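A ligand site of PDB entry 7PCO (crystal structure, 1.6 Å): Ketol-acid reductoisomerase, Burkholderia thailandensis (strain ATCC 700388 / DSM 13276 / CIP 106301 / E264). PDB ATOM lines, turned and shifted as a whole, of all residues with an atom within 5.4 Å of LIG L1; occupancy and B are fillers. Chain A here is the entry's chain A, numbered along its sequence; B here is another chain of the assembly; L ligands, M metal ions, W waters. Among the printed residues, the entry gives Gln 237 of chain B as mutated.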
ATOM      1  N   GLY A  30      -6.265  20.436  25.500  1.00  0.00           N
ATOM      2  CA  GLY A  30      -5.708  21.571  24.755  1.00  0.00           C
ATOM      3  C   GLY A  30      -5.687  22.795  25.627  1.00  0.00           C
ATOM      4  O   GLY A  30      -6.456  22.867  26.592  1.00  0.00           O
ATOM      5  N   TYR A  31      -4.753  23.696  25.358  1.00  0.00           N
ATOM      6  CA  TYR A  31      -4.592  24.941  26.137  1.00  0.00           C
ATOM      7  C   TYR A  31      -4.092  25.997  25.146  1.00  0.00           C
ATOM      8  O   TYR A  31      -3.290  26.865  25.506  1.00  0.00           O
ATOM      9  CB  TYR A  31      -3.682  24.689  27.341  1.00  0.00           C
ATOM     10  CG  TYR A  31      -3.760  25.744  28.409  1.00  0.00           C
ATOM     11  CD1 TYR A  31      -4.821  25.786  29.292  1.00  0.00           C
ATOM     12  CD2 TYR A  31      -2.774  26.720  28.522  1.00  0.00           C
ATOM     13  CE1 TYR A  31      -4.891  26.744  30.290  1.00  0.00           C
ATOM     14  CE2 TYR A  31      -2.824  27.683  29.518  1.00  0.00           C
ATOM     15  CZ  TYR A  31      -3.906  27.715  30.383  1.00  0.00           C
ATOM     16  OH  TYR A  31      -3.960  28.678  31.338  1.00  0.00           O
ATOM     17  N   GLY A  32      -4.590  25.876  23.914  1.00  0.00           N
ATOM     18  CA  GLY A  32      -4.322  26.821  22.825  1.00  0.00           C
ATOM     19  C   GLY A  32      -5.275  27.992  22.852  1.00  0.00           C
ATOM     20  O   GLY A  32      -5.722  28.463  23.947  1.00  0.00           O
ATOM     21  N   ILE A  33      -5.561  28.484  21.657  1.00  0.00           N
ATOM     22  CA  ILE A  33      -6.324  29.750  21.468  1.00  0.00           C
ATOM     23  C   ILE A  33      -7.660  29.599  22.223  1.00  0.00           C
ATOM     24  O   ILE A  33      -8.005  30.474  23.068  1.00  0.00           O
ATOM     25  CB  ILE A  33      -6.505  30.038  19.965  1.00  0.00           C
ATOM     26  CG1 ILE A  33      -5.167  30.322  19.283  1.00  0.00           C
ATOM     27  CG2 ILE A  33      -7.480  31.193  19.750  1.00  0.00           C
ATOM     28  CD1 ILE A  33      -5.065  29.836  17.848  1.00  0.00           C
ATOM     29  N   GLN A  34      -8.337  28.477  21.996  1.00  0.00           N
ATOM     30  CA  GLN A  34      -9.641  28.203  22.633  1.00  0.00           C
ATOM     31  C   GLN A  34      -9.436  27.593  24.034  1.00  0.00           C
ATOM     32  O   GLN A  34     -10.077  28.074  24.992  1.00  0.00           O
ATOM     33  CB  GLN A  34     -10.478  27.316  21.724  1.00  0.00           C
ATOM     34  CG  GLN A  34     -11.010  28.051  20.516  1.00  0.00           C
ATOM     35  CD  GLN A  34     -11.950  29.186  20.858  1.00  0.00           C
ATOM     36  OE1 GLN A  34     -12.771  29.081  21.763  1.00  0.00           O
ATOM     37  NE2 GLN A  34     -11.801  30.308  20.167  1.00  0.00           N
ATOM     38  N   GLY A  35      -8.573  26.591  24.178  1.00  0.00           N
ATOM     39  CA  GLY A  35      -8.431  25.861  25.455  1.00  0.00           C
ATOM     40  C   GLY A  35      -8.084  26.800  26.591  1.00  0.00           C
ATOM     41  O   GLY A  35      -8.621  26.650  27.687  1.00  0.00           O
ATOM     42  N   ASN A  53      -3.014  17.694  28.253  1.00  0.00           N
ATOM     43  CA  ASN A  53      -2.138  18.261  27.191  1.00  0.00           C
ATOM     44  C   ASN A  53      -0.927  17.355  26.948  1.00  0.00           C
ATOM     45  O   ASN A  53      -0.450  16.721  27.910  1.00  0.00           O
ATOM     46  CB  ASN A  53      -1.712  19.693  27.524  1.00  0.00           C
ATOM     47  CG  ASN A  53      -1.374  20.524  26.304  1.00  0.00           C
ATOM     48  OD1 ASN A  53      -2.223  21.249  25.791  1.00  0.00           O
ATOM     49  ND2 ASN A  53      -0.139  20.425  25.816  1.00  0.00           N
ATOM     50  N   ILE A  54      -0.502  17.277  25.683  1.00  0.00           N
ATOM     51  CA  ILE A  54       0.752  16.600  25.252  1.00  0.00           C
ATOM     52  C   ILE A  54       1.938  17.399  25.805  1.00  0.00           C
ATOM     53  O   ILE A  54       1.762  18.522  26.330  1.00  0.00           O
ATOM     54  CB  ILE A  54       0.806  16.397  23.715  1.00  0.00           C
ATOM     55  CG1 ILE A  54       0.904  17.708  22.932  1.00  0.00           C
ATOM     56  CG2 ILE A  54      -0.377  15.544  23.256  1.00  0.00           C
ATOM     57  CD1 ILE A  54       1.176  17.526  21.441  1.00  0.00           C
ATOM     58  N   ASP A  56       4.375  19.684  25.389  1.00  0.00           N
ATOM     59  CA  ASP A  56       4.785  20.869  24.578  1.00  0.00           C
ATOM     60  C   ASP A  56       4.653  22.148  25.424  1.00  0.00           C
ATOM     61  O   ASP A  56       4.407  22.043  26.630  1.00  0.00           O
ATOM     62  CB  ASP A  56       4.026  20.934  23.234  1.00  0.00           C
ATOM     63  CG  ASP A  56       2.537  21.213  23.376  1.00  0.00           C
ATOM     64  OD1 ASP A  56       2.128  21.622  24.473  1.00  0.00           O
ATOM     65  OD2 ASP A  56       1.804  21.047  22.360  1.00  0.00           O
ATOM     66  N   TYR A  58       2.474  24.360  25.706  1.00  0.00           N
ATOM     67  CA  TYR A  58       1.132  24.641  26.250  1.00  0.00           C
ATOM     68  C   TYR A  58       0.969  23.955  27.613  1.00  0.00           C
ATOM     69  O   TYR A  58       0.283  24.493  28.500  1.00  0.00           O
ATOM     70  CB  TYR A  58       0.064  24.218  25.247  1.00  0.00           C
ATOM     71  CG  TYR A  58       0.101  24.928  23.925  1.00  0.00           C
ATOM     72  CD1 TYR A  58       0.769  24.375  22.838  1.00  0.00           C
ATOM     73  CD2 TYR A  58      -0.545  26.144  23.732  1.00  0.00           C
ATOM     74  CE1 TYR A  58       0.766  24.995  21.600  1.00  0.00           C
ATOM     75  CE2 TYR A  58      -0.541  26.776  22.491  1.00  0.00           C
ATOM     76  CZ  TYR A  58       0.105  26.198  21.421  1.00  0.00           C
ATOM     77  OH  TYR A  58       0.092  26.787  20.200  1.00  0.00           O
ATOM     78  N   ILE A  72      -3.443  13.634  28.380  1.00  0.00           N
ATOM     79  CA  ILE A  72      -4.859  13.714  27.927  1.00  0.00           C
ATOM     80  C   ILE A  72      -5.640  12.547  28.536  1.00  0.00           C
ATOM     81  O   ILE A  72      -6.722  12.804  29.104  1.00  0.00           O
ATOM     82  CB  ILE A  72      -4.926  13.760  26.380  1.00  0.00           C
ATOM     83  CG1 ILE A  72      -4.331  15.070  25.851  1.00  0.00           C
ATOM     84  CG2 ILE A  72      -6.358  13.543  25.902  1.00  0.00           C
ATOM     85  CD1 ILE A  72      -4.155  15.124  24.352  1.00  0.00           C
ATOM     86  N   LEU A  84     -12.737  18.937  23.674  1.00  0.00           N
ATOM     87  CA  LEU A  84     -11.602  18.586  22.786  1.00  0.00           C
ATOM     88  C   LEU A  84     -11.164  19.839  22.009  1.00  0.00           C
ATOM     89  O   LEU A  84     -11.653  20.074  20.892  1.00  0.00           O
ATOM     90  CB  LEU A  84     -12.027  17.445  21.863  1.00  0.00           C
ATOM     91  CG  LEU A  84     -10.947  16.897  20.929  1.00  0.00           C
ATOM     92  CD1 LEU A  84      -9.658  16.568  21.692  1.00  0.00           C
ATOM     93  CD2 LEU A  84     -11.467  15.679  20.182  1.00  0.00           C
ATOM     94  N   LEU A  85     -10.250  20.616  22.591  1.00  0.00           N
ATOM     95  CA  LEU A  85      -9.824  21.925  22.039  1.00  0.00           C
ATOM     96  C   LEU A  85      -8.381  21.820  21.532  1.00  0.00           C
ATOM     97  O   LEU A  85      -7.499  22.594  21.992  1.00  0.00           O
ATOM     98  CB  LEU A  85     -10.081  23.015  23.077  1.00  0.00           C
ATOM     99  CG  LEU A  85     -11.554  23.088  23.521  1.00  0.00           C
ATOM    100  CD1 LEU A  85     -11.753  24.103  24.625  1.00  0.00           C
ATOM    101  CD2 LEU A  85     -12.482  23.383  22.349  1.00  0.00           C
ATOM    102  N   ILE A  86      -8.183  20.938  20.562  1.00  0.00           N
ATOM    103  CA  ILE A  86      -6.896  20.739  19.827  1.00  0.00           C
ATOM    104  C   ILE A  86      -7.213  20.808  18.338  1.00  0.00           C
ATOM    105  O   ILE A  86      -8.382  20.728  17.940  1.00  0.00           O
ATOM    106  CB  ILE A  86      -6.226  19.407  20.240  1.00  0.00           C
ATOM    107  CG1 ILE A  86      -6.967  18.195  19.677  1.00  0.00           C
ATOM    108  CG2 ILE A  86      -6.106  19.349  21.756  1.00  0.00           C
ATOM    109  CD1 ILE A  86      -6.275  16.863  19.904  1.00  0.00           C
ATOM    110  N   PRO A  87      -6.196  21.010  17.464  1.00  0.00           N
ATOM    111  CA  PRO A  87      -6.419  21.097  16.029  1.00  0.00           C
ATOM    112  C   PRO A  87      -7.229  19.909  15.473  1.00  0.00           C
ATOM    113  O   PRO A  87      -7.008  18.776  15.894  1.00  0.00           O
ATOM    114  CB  PRO A  87      -4.982  21.109  15.475  1.00  0.00           C
ATOM    115  CG  PRO A  87      -4.209  21.775  16.581  1.00  0.00           C
ATOM    116  CD  PRO A  87      -4.771  21.126  17.822  1.00  0.00           C
ATOM    117  N   ASP A  88      -8.120  20.202  14.536  1.00  0.00           N
ATOM    118  CA  ASP A  88      -9.126  19.225  14.046  1.00  0.00           C
ATOM    119  C   ASP A  88      -8.470  17.967  13.467  1.00  0.00           C
ATOM    120  O   ASP A  88      -8.985  16.873  13.749  1.00  0.00           O
ATOM    121  CB  ASP A  88     -10.081  19.931  13.090  1.00  0.00           C
ATOM    122  CG  ASP A  88     -10.643  21.179  13.738  1.00  0.00           C
ATOM    123  OD1 ASP A  88     -11.518  21.028  14.604  1.00  0.00           O
ATOM    124  OD2 ASP A  88     -10.154  22.282  13.435  1.00  0.00           O
ATOM    125  N   ALA A  90      -5.956  16.459  14.386  1.00  0.00           N
ATOM    126  CA  ALA A  90      -5.432  15.638  15.501  1.00  0.00           C
ATOM    127  C   ALA A  90      -6.552  14.888  16.247  1.00  0.00           C
ATOM    128  O   ALA A  90      -6.214  14.008  17.046  1.00  0.00           O
ATOM    129  CB  ALA A  90      -4.655  16.497  16.461  1.00  0.00           C
ATOM    130  N   HIS A  91      -7.826  15.211  15.989  1.00  0.00           N
ATOM    131  CA  HIS A  91      -8.977  14.663  16.773  1.00  0.00           C
ATOM    132  C   HIS A  91      -9.052  13.138  16.660  1.00  0.00           C
ATOM    133  O   HIS A  91      -9.263  12.499  17.707  1.00  0.00           O
ATOM    134  CB  HIS A  91     -10.317  15.268  16.331  1.00  0.00           C
ATOM    135  CG  HIS A  91     -10.528  16.695  16.727  1.00  0.00           C
ATOM    136  ND1 HIS A  91     -11.766  17.301  16.649  1.00  0.00           N
ATOM    137  CD2 HIS A  91      -9.686  17.599  17.252  1.00  0.00           C
ATOM    138  CE1 HIS A  91     -11.665  18.548  17.070  1.00  0.00           C
ATOM    139  NE2 HIS A  91     -10.380  18.764  17.443  1.00  0.00           N
ATOM    140  N   VAL A  94      -6.355  11.142  18.788  1.00  0.00           N
ATOM    141  CA  VAL A  94      -6.533  11.462  20.244  1.00  0.00           C
ATOM    142  C   VAL A  94      -7.853  10.844  20.733  1.00  0.00           C
ATOM    143  O   VAL A  94      -7.864  10.301  21.852  1.00  0.00           O
ATOM    144  CB  VAL A  94      -6.446  12.975  20.534  1.00  0.00           C
ATOM    145  CG1 VAL A  94      -6.849  13.308  21.966  1.00  0.00           C
ATOM    146  CG2 VAL A  94      -5.032  13.484  20.249  1.00  0.00           C
ATOM    147  N   ALA A 112     -15.506  21.934  19.290  1.00  0.00           N
ATOM    148  CA  ALA A 112     -15.758  23.379  19.078  1.00  0.00           C
ATOM    149  C   ALA A 112     -15.829  23.693  17.594  1.00  0.00           C
ATOM    150  O   ALA A 112     -15.845  24.870  17.247  1.00  0.00           O
ATOM    151  CB  ALA A 112     -14.686  24.194  19.766  1.00  0.00           C
ATOM    152  N   HIS A 113     -15.891  22.664  16.742  1.00  0.00           N
ATOM    153  CA  HIS A 113     -15.985  22.760  15.267  1.00  0.00           C
ATOM    154  C   HIS A 113     -16.471  21.402  14.766  1.00  0.00           C
ATOM    155  O   HIS A 113     -16.043  20.375  15.347  1.00  0.00           O
ATOM    156  CB  HIS A 113     -14.621  23.180  14.686  1.00  0.00           C
ATOM    157  CG  HIS A 113     -14.521  23.288  13.200  1.00  0.00           C
ATOM    158  ND1 HIS A 113     -15.450  23.933  12.421  1.00  0.00           N
ATOM    159  CD2 HIS A 113     -13.493  22.971  12.371  1.00  0.00           C
ATOM    160  CE1 HIS A 113     -15.039  23.949  11.166  1.00  0.00           C
ATOM    161  NE2 HIS A 113     -13.846  23.375  11.106  1.00  0.00           N
ATOM    162  N   ALA A 134     -19.444  25.685  19.451  1.00  0.00           N
ATOM    163  CA  ALA A 134     -18.506  26.292  18.489  1.00  0.00           C
ATOM    164  C   ALA A 134     -18.538  27.807  18.651  1.00  0.00           C
ATOM    165  O   ALA A 134     -19.441  28.460  18.126  1.00  0.00           O
ATOM    166  CB  ALA A 134     -18.872  25.887  17.089  1.00  0.00           C
ATOM    167  N   PRO A 135     -17.564  28.390  19.386  1.00  0.00           N
ATOM    168  CA  PRO A 135     -17.477  29.838  19.517  1.00  0.00           C
ATOM    169  C   PRO A 135     -17.244  30.502  18.155  1.00  0.00           C
ATOM    170  O   PRO A 135     -16.666  29.900  17.268  1.00  0.00           O
ATOM    171  CB  PRO A 135     -16.297  30.060  20.468  1.00  0.00           C
ATOM    172  CG  PRO A 135     -16.143  28.712  21.175  1.00  0.00           C
ATOM    173  CD  PRO A 135     -16.475  27.703  20.095  1.00  0.00           C
ATOM    174  N   MET A 137     -15.650  33.461  17.831  1.00  0.00           N
ATOM    175  CA  MET A 137     -14.577  34.458  18.119  1.00  0.00           C
ATOM    176  C   MET A 137     -13.345  33.691  18.603  1.00  0.00           C
ATOM    177  O   MET A 137     -13.517  32.599  19.166  1.00  0.00           O
ATOM    178  CB  MET A 137     -15.071  35.405  19.212  1.00  0.00           C
ATOM    179  CG  MET A 137     -14.142  36.533  19.569  1.00  0.00           C
ATOM    180  SD  MET A 137     -13.705  37.629  18.203  1.00  0.00           S
ATOM    181  CE  MET A 137     -15.248  38.484  17.867  1.00  0.00           C
ATOM    182  N   TYR A 138     -12.168  34.267  18.417  1.00  0.00           N
ATOM    183  CA  TYR A 138     -10.900  33.689  18.939  1.00  0.00           C
ATOM    184  C   TYR A 138     -10.756  34.028  20.436  1.00  0.00           C
ATOM    185  O   TYR A 138     -11.607  34.708  21.021  1.00  0.00           O
ATOM    186  CB  TYR A 138      -9.725  34.056  18.020  1.00  0.00           C
ATOM    187  CG  TYR A 138      -9.525  35.488  17.615  1.00  0.00           C
ATOM    188  CD1 TYR A 138      -8.718  36.340  18.349  1.00  0.00           C
ATOM    189  CD2 TYR A 138     -10.068  35.971  16.433  1.00  0.00           C
ATOM    190  CE1 TYR A 138      -8.474  37.646  17.939  1.00  0.00           C
ATOM    191  CE2 TYR A 138      -9.836  37.281  16.013  1.00  0.00           C
ATOM    192  CZ  TYR A 138      -9.021  38.105  16.753  1.00  0.00           C
ATOM    193  OH  TYR A 138      -8.773  39.385  16.319  1.00  0.00           O
ATOM    194  N   GLY A 139      -9.703  33.512  21.046  1.00  0.00           N
ATOM    195  CA  GLY A 139      -9.573  33.393  22.514  1.00  0.00           C
ATOM    196  C   GLY A 139      -9.469  34.718  23.246  1.00  0.00           C
ATOM    197  O   GLY A 139     -10.146  34.866  24.292  1.00  0.00           O
ATOM    198  N   GLN B 237     -16.032  39.095  14.513  1.00  0.00           N
ATOM    199  CA  GLN B 237     -14.736  38.418  14.276  1.00  0.00           C
ATOM    200  C   GLN B 237     -13.970  39.082  13.125  1.00  0.00           C
ATOM    201  O   GLN B 237     -12.743  39.265  13.271  1.00  0.00           O
ATOM    202  CB  GLN B 237     -14.854  36.934  13.970  1.00  0.00           C
ATOM    203  CG  GLN B 237     -13.489  36.283  13.858  1.00  0.00           C
ATOM    204  CD  GLN B 237     -13.577  34.781  13.975  1.00  0.00           C
ATOM    205  OE1 GLN B 237     -14.064  34.105  13.074  1.00  0.00           O
ATOM    206  NE2 GLN B 237     -13.083  34.256  15.076  1.00  0.00           N
ATOM    207  N   GLN B 257      -3.838  33.569  15.817  1.00  0.00           N
ATOM    208  CA  GLN B 257      -5.173  33.404  16.452  1.00  0.00           C
ATOM    209  C   GLN B 257      -5.976  32.322  15.739  1.00  0.00           C
ATOM    210  O   GLN B 257      -7.021  31.935  16.277  1.00  0.00           O
ATOM    211  CB  GLN B 257      -5.979  34.704  16.433  1.00  0.00           C
ATOM    212  CG  GLN B 257      -5.307  35.855  17.157  1.00  0.00           C
ATOM    213  CD  GLN B 257      -5.244  35.691  18.658  1.00  0.00           C
ATOM    214  OE1 GLN B 257      -5.248  34.592  19.204  1.00  0.00           O
ATOM    215  NE2 GLN B 257      -5.183  36.815  19.356  1.00  0.00           N
ATOM    216  N   GLY B 258      -5.537  31.885  14.565  1.00  0.00           N
ATOM    217  CA  GLY B 258      -6.258  30.858  13.795  1.00  0.00           C
ATOM    218  C   GLY B 258      -5.812  29.451  14.163  1.00  0.00           C
ATOM    219  O   GLY B 258      -4.595  29.189  14.339  1.00  0.00           O
ATOM    220  N   SER B 259      -6.772  28.535  14.252  1.00  0.00           N
ATOM    221  CA  SER B 259      -6.531  27.081  14.333  1.00  0.00           C
ATOM    222  C   SER B 259      -5.719  26.670  13.114  1.00  0.00           C
ATOM    223  O   SER B 259      -5.724  27.343  12.080  1.00  0.00           O
ATOM    224  CB  SER B 259      -7.841  26.338  14.419  1.00  0.00           C
ATOM    225  OG  SER B 259      -8.457  26.290  13.146  1.00  0.00           O
ATOM    226  N   PRO B 260      -4.953  25.566  13.163  1.00  0.00           N
ATOM    227  CA  PRO B 260      -4.249  25.107  11.971  1.00  0.00           C
ATOM    228  C   PRO B 260      -5.212  24.881  10.795  1.00  0.00           C
ATOM    229  O   PRO B 260      -4.829  25.132   9.684  1.00  0.00           O
ATOM    230  CB  PRO B 260      -3.571  23.815  12.456  1.00  0.00           C
ATOM    231  CG  PRO B 260      -3.341  24.099  13.931  1.00  0.00           C
ATOM    232  CD  PRO B 260      -4.600  24.800  14.376  1.00  0.00           C
ATOM    233  N   THR B 261      -6.452  24.453  11.064  1.00  0.00           N
ATOM    234  CA  THR B 261      -7.500  24.255  10.040  1.00  0.00           C
ATOM    235  C   THR B 261      -7.754  25.584   9.331  1.00  0.00           C
ATOM    236  O   THR B 261      -7.776  25.621   8.082  1.00  0.00           O
ATOM    237  CB  THR B 261      -8.793  23.706  10.667  1.00  0.00           C
ATOM    238  OG1 THR B 261      -8.434  22.531  11.398  1.00  0.00           O
ATOM    239  CG2 THR B 261      -9.871  23.427   9.652  1.00  0.00           C
HETATM  240  P1  LIG L   1      -4.414  25.672  18.635  1.00  0.00           P
HETATM  241  O1  LIG L   1      -3.629  25.573  17.368  1.00  0.00           O
HETATM  242  O2  LIG L   1      -4.304  26.855  19.543  1.00  0.00           O
HETATM  243  O3  LIG L   1      -4.207  24.335  19.471  1.00  0.00           O
HETATM  244  C1  LIG L   1      -3.048  24.209  20.317  1.00  0.00           C
HETATM  245  C2  LIG L   1      -3.355  23.155  21.350  1.00  0.00           C
HETATM  246  O4  LIG L   1      -3.517  21.882  20.691  1.00  0.00           O
HETATM  247  C3  LIG L   1      -2.281  22.933  22.416  1.00  0.00           C
HETATM  248  O5  LIG L   1      -2.871  22.576  23.664  1.00  0.00           O
HETATM  249  C4  LIG L   1      -1.487  21.778  21.829  1.00  0.00           C
HETATM  250  O6  LIG L   1      -0.778  21.071  22.827  1.00  0.00           O
HETATM  251  C5  LIG L   1      -2.617  20.945  21.239  1.00  0.00           C
HETATM  252  N1  LIG L   1      -2.232  19.999  20.203  1.00  0.00           N
HETATM  253  C6  LIG L   1      -1.750  20.292  18.954  1.00  0.00           C
HETATM  254  N2  LIG L   1      -1.521  19.236  18.217  1.00  0.00           N
HETATM  255  C7  LIG L   1      -1.892  18.166  19.010  1.00  0.00           C
HETATM  256  C8  LIG L   1      -1.878  16.773  18.801  1.00  0.00           C
HETATM  257  N3  LIG L   1      -1.482  16.204  17.669  1.00  0.00           N
HETATM  258  N4  LIG L   1      -2.313  15.985  19.810  1.00  0.00           N
HETATM  259  C9  LIG L   1      -2.712  16.566  20.950  1.00  0.00           C
HETATM  260  N5  LIG L   1      -2.759  17.854  21.267  1.00  0.00           N
HETATM  261  C10 LIG L   1      -2.329  18.616  20.243  1.00  0.00           C
HETATM  262  O7  LIG L   1      -5.947  25.443  18.247  1.00  0.00           O
HETATM  263  P2  LIG L   1      -7.332  26.226  18.505  1.00  0.00           P
HETATM  264  O8  LIG L   1      -7.490  27.319  17.506  1.00  0.00           O
HETATM  265  O9  LIG L   1      -7.383  26.544  19.975  1.00  0.00           O
HETATM  266  O10 LIG L   1      -8.360  25.056  18.090  1.00  0.00           O
HETATM  267  C11 LIG L   1      -8.895  24.104  19.018  1.00  0.00           C
HETATM  268  C12 LIG L   1     -10.265  23.729  18.511  1.00  0.00           C
HETATM  269  O11 LIG L   1     -11.084  24.914  18.570  1.00  0.00           O
HETATM  270  C13 LIG L   1     -10.355  23.244  17.055  1.00  0.00           C
HETATM  271  O12 LIG L   1     -11.323  22.220  16.891  1.00  0.00           O
HETATM  272  C14 LIG L   1     -10.745  24.523  16.302  1.00  0.00           C
HETATM  273  O13 LIG L   1     -11.381  24.325  15.053  1.00  0.00           O
HETATM  274  C15 LIG L   1     -11.699  25.108  17.334  1.00  0.00           C
HETATM  275  N6  LIG L   1     -11.957  26.566  17.191  1.00  0.00           N
HETATM  276  C16 LIG L   1     -10.925  27.478  17.090  1.00  0.00           C
HETATM  277  C17 LIG L   1     -11.192  28.835  17.186  1.00  0.00           C
HETATM  278  C18 LIG L   1     -10.122  29.903  17.161  1.00  0.00           C
HETATM  279  O14 LIG L   1     -10.482  31.077  17.179  1.00  0.00           O
HETATM  280  N7  LIG L   1      -8.853  29.539  17.080  1.00  0.00           N
HETATM  281  C19 LIG L   1     -12.529  29.252  17.258  1.00  0.00           C
HETATM  282  C20 LIG L   1     -13.529  28.318  17.312  1.00  0.00           C
HETATM  283  C21 LIG L   1     -13.229  26.986  17.290  1.00  0.00           C
HETATM  284  C1  LG2 L   2     -11.829  29.670  14.031  1.00  0.00           C
HETATM  285  C2  LG2 L   2     -11.932  31.124  13.954  1.00  0.00           C
HETATM  286  C3  LG2 L   2     -11.789  31.658  12.502  1.00  0.00           C
HETATM  287  C4  LG2 L   2     -10.379  33.917  12.551  1.00  0.00           C
HETATM  288  O1  LG2 L   2      -9.436  29.500  13.843  1.00  0.00           O
HETATM  289  C5  LG2 L   2     -10.498  28.943  13.608  1.00  0.00           C
HETATM  290  O2  LG2 L   2     -10.642  27.832  13.138  1.00  0.00           O
HETATM  291  O3  LG2 L   2     -12.939  29.156  13.358  1.00  0.00           O
HETATM  292  O4  LG2 L   2     -13.244  31.491  14.508  1.00  0.00           O
HETATM  293  C6  LG2 L   2     -10.455  32.427  12.706  1.00  0.00           C
HETATM  294  C7  LG2 L   2     -10.064  34.296  11.136  1.00  0.00           C
HETATM  295  C8  LG2 L   2      -9.234  34.486  13.383  1.00  0.00           C
HETATM  296 MG    MG M   1     -12.582  27.460  12.288  1.00  0.00          MG
HETATM  297 MG    MG M   2     -14.600  30.222  13.330  1.00  0.00          MG
HETATM  298  O   HOH W   1      -1.392  23.804  17.292  1.00  0.00           O
HETATM  299  O   HOH W   2     -13.070  26.235  13.820  1.00  0.00           O
HETATM  300  O   HOH W   3     -15.649  26.433  14.852  1.00  0.00           O
HETATM  301  O   HOH W   4      -1.415  19.607  15.449  1.00  0.00           O
HETATM  302  O   HOH W   5     -15.520  29.261  14.905  1.00  0.00           O
HETATM  303  O   HOH W   6     -12.911  21.014  18.799  1.00  0.00           O
HETATM  304  O   HOH W   7      -2.813  27.669  15.870  1.00  0.00           O
HETATM  305  O   HOH W   8      -6.943  25.222  22.213  1.00  0.00           O
HETATM  306  O   HOH W   9      -2.052  28.343  19.746  1.00  0.00           O
HETATM  307  O   HOH W  10      -1.395  13.377  20.633  1.00  0.00           O
HETATM  308  O   HOH W  11      -2.392  18.643  23.924  1.00  0.00           O
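Water W8 lies within hydrogen-bond range of an oxygen (O9) of LIG L1 (2.6 Å), the backbone carbonyl oxygen (O) of Leu 85 (2.7 Å), the backbone NH (N) of Gly 35 (2.9 Å) and the backbone NH (N) of Gly 32 (3.0 Å).
Water W7 bridges an oxygen (O1) of LIG L1 and the backbone carbonyl oxygen of Gly 258 of chain B.
Water W9 bridges the side-chain hydroxyl of Tyr 58 (2.7 Å) and an oxygen (O2) of LIG L1 (2.7 Å).
Water W6 lies within hydrogen-bond range of the backbone carbonyl oxygen (O) of Leu 84 (2.6 Å), an oxygen (O12) of LIG L1 (2.8 Å) and the backbone NH (N) of Ala 112 (2.8 Å).
Water W11 lies within hydrogen-bond range of a nitrogen (N5) of LIG L1, the backbone NH (N) of Ile 54 and the side-chain amide oxygen (OD1) of Asn 53.
Water W3 bridges O of Ala 112 (2.9 Å) and ND1 of His 113 (3.5 Å).
Residues that only touch LIG L1: Tyr 138 (3.2 Å), Gly 30 (3.2 Å), Pro 87 (3.2 Å), Pro 260 of chain B (3.2 Å), Ser 259 of chain B (3.3 Å), Gly 32 (3.3 Å), Ala 112 (3.4 Å), Tyr 58 (3.4 Å), Ala 90 (3.4 Å), Leu 85 (3.4 Å), Ile 54 (3.4 Å), His 113 (3.5 Å), Pro 135 (3.5 Å), His 91 (3.6 Å), Val 94 (3.7 Å), Met 137 (3.9 Å) and Ile 72 (3.97 Å).
Hydrophobic or aromatic side chains that line LIG L1: Ile 33, Ile 54, Tyr 58, Ile 72, Ile 86, Pro 87, Ala 90, His 91, Val 94, Ala 112, His 113, Tyr 138 and Pro 260 of chain B.
25 residues have an atom within 4 Å of LIG L1: Gly 30, Tyr 31, Gly 32, Ile 33, Gln 34, Asn 53, Ile 54, Asp 56, Tyr 58, Ile 72, Leu 85, Ile 86, Pro 87, Asp 88, Ala 90, His 91, Val 94, Ala 112, His 113, Pro 135, Met 137, Tyr 138, Gln 257 of chain B, Ser 259 of chain B and Pro 260 of chain B.
Along chain A the residues within 4 Å of LIG L1 span positions 30 to 138.
An oxygen (O1) of LG2 L2 is in hydrogen-bond range of a nitrogen (N7) of LIG L1, 3.3 Å away.
N of Thr 261 of chain B sits close to OG of Ser 259 of chain B, at 3.4 Å.
The backbone NH (N) of Tyr 58 sits at hydrogen-bond distance from the side-chain carboxylate (OD1) of Asp 56 (3.0 Å).
The side-chain carboxylate (OD1) of Asp 56 is in hydrogen-bond range of the side-chain amide nitrogen (ND2) of Asn 53.
The side-chain amide nitrogen (NE2) of Gln 237 of chain B lies close to the backbone NH (N) of Tyr 138.
O of Met 137 is in hydrogen-bond range of NE2 of Gln 34 (3.0 Å).
The backbone carbonyl oxygen (O) of Ile 86 sits at hydrogen-bond distance from a ring nitrogen (NE2) of His 91.
The side-chain hydroxyl (OG1) of Thr 261 of chain B is in hydrogen-bond range of the side-chain carboxylate (OD2) of Asp 88 (2.7 Å).
N of Ile 33 is in hydrogen-bond range of O2 of LIG L1, 3.0 Å away.
An oxygen (O1) of LG2 L2 is in hydrogen-bond range of the backbone NH (N) of Ser 259 of chain B (2.9 Å).
An oxygen (O1) of LG2 L2 lies close to the side-chain hydroxyl (OG) of Ser 259 of chain B (3.4 Å).
The side-chain carboxylate of Asp 88 lies within hydrogen-bond range of an oxygen (O12) of LIG L1, 2.6 Å away.
The backbone NH (N) of Gln 34 sits at hydrogen-bond distance from an oxygen (O9) of LIG L1, at 3.0 Å.
O5 of LIG L1 is in hydrogen-bond range of OD1 of Asn 53 (2.6 Å).
N7 of LIG L1 sits at hydrogen-bond distance from O of Gln 257 of chain B (3.1 Å).
NE2 of Gln 34 sits close to O14 of LIG L1 (3.4 Å).
The side-chain carboxylate of Asp 56 lies within hydrogen-bond range of an oxygen (O6) of LIG L1 (2.6 Å).
NE2 of Gln 237 of chain B sits close to O4 of LG2 L2, 2.8 Å away.
O12 of LIG L1 sits close to O of Ile 86 (3.5 Å).
N of Tyr 31 is in hydrogen-bond range of O5 of LIG L1, 2.8 Å away.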
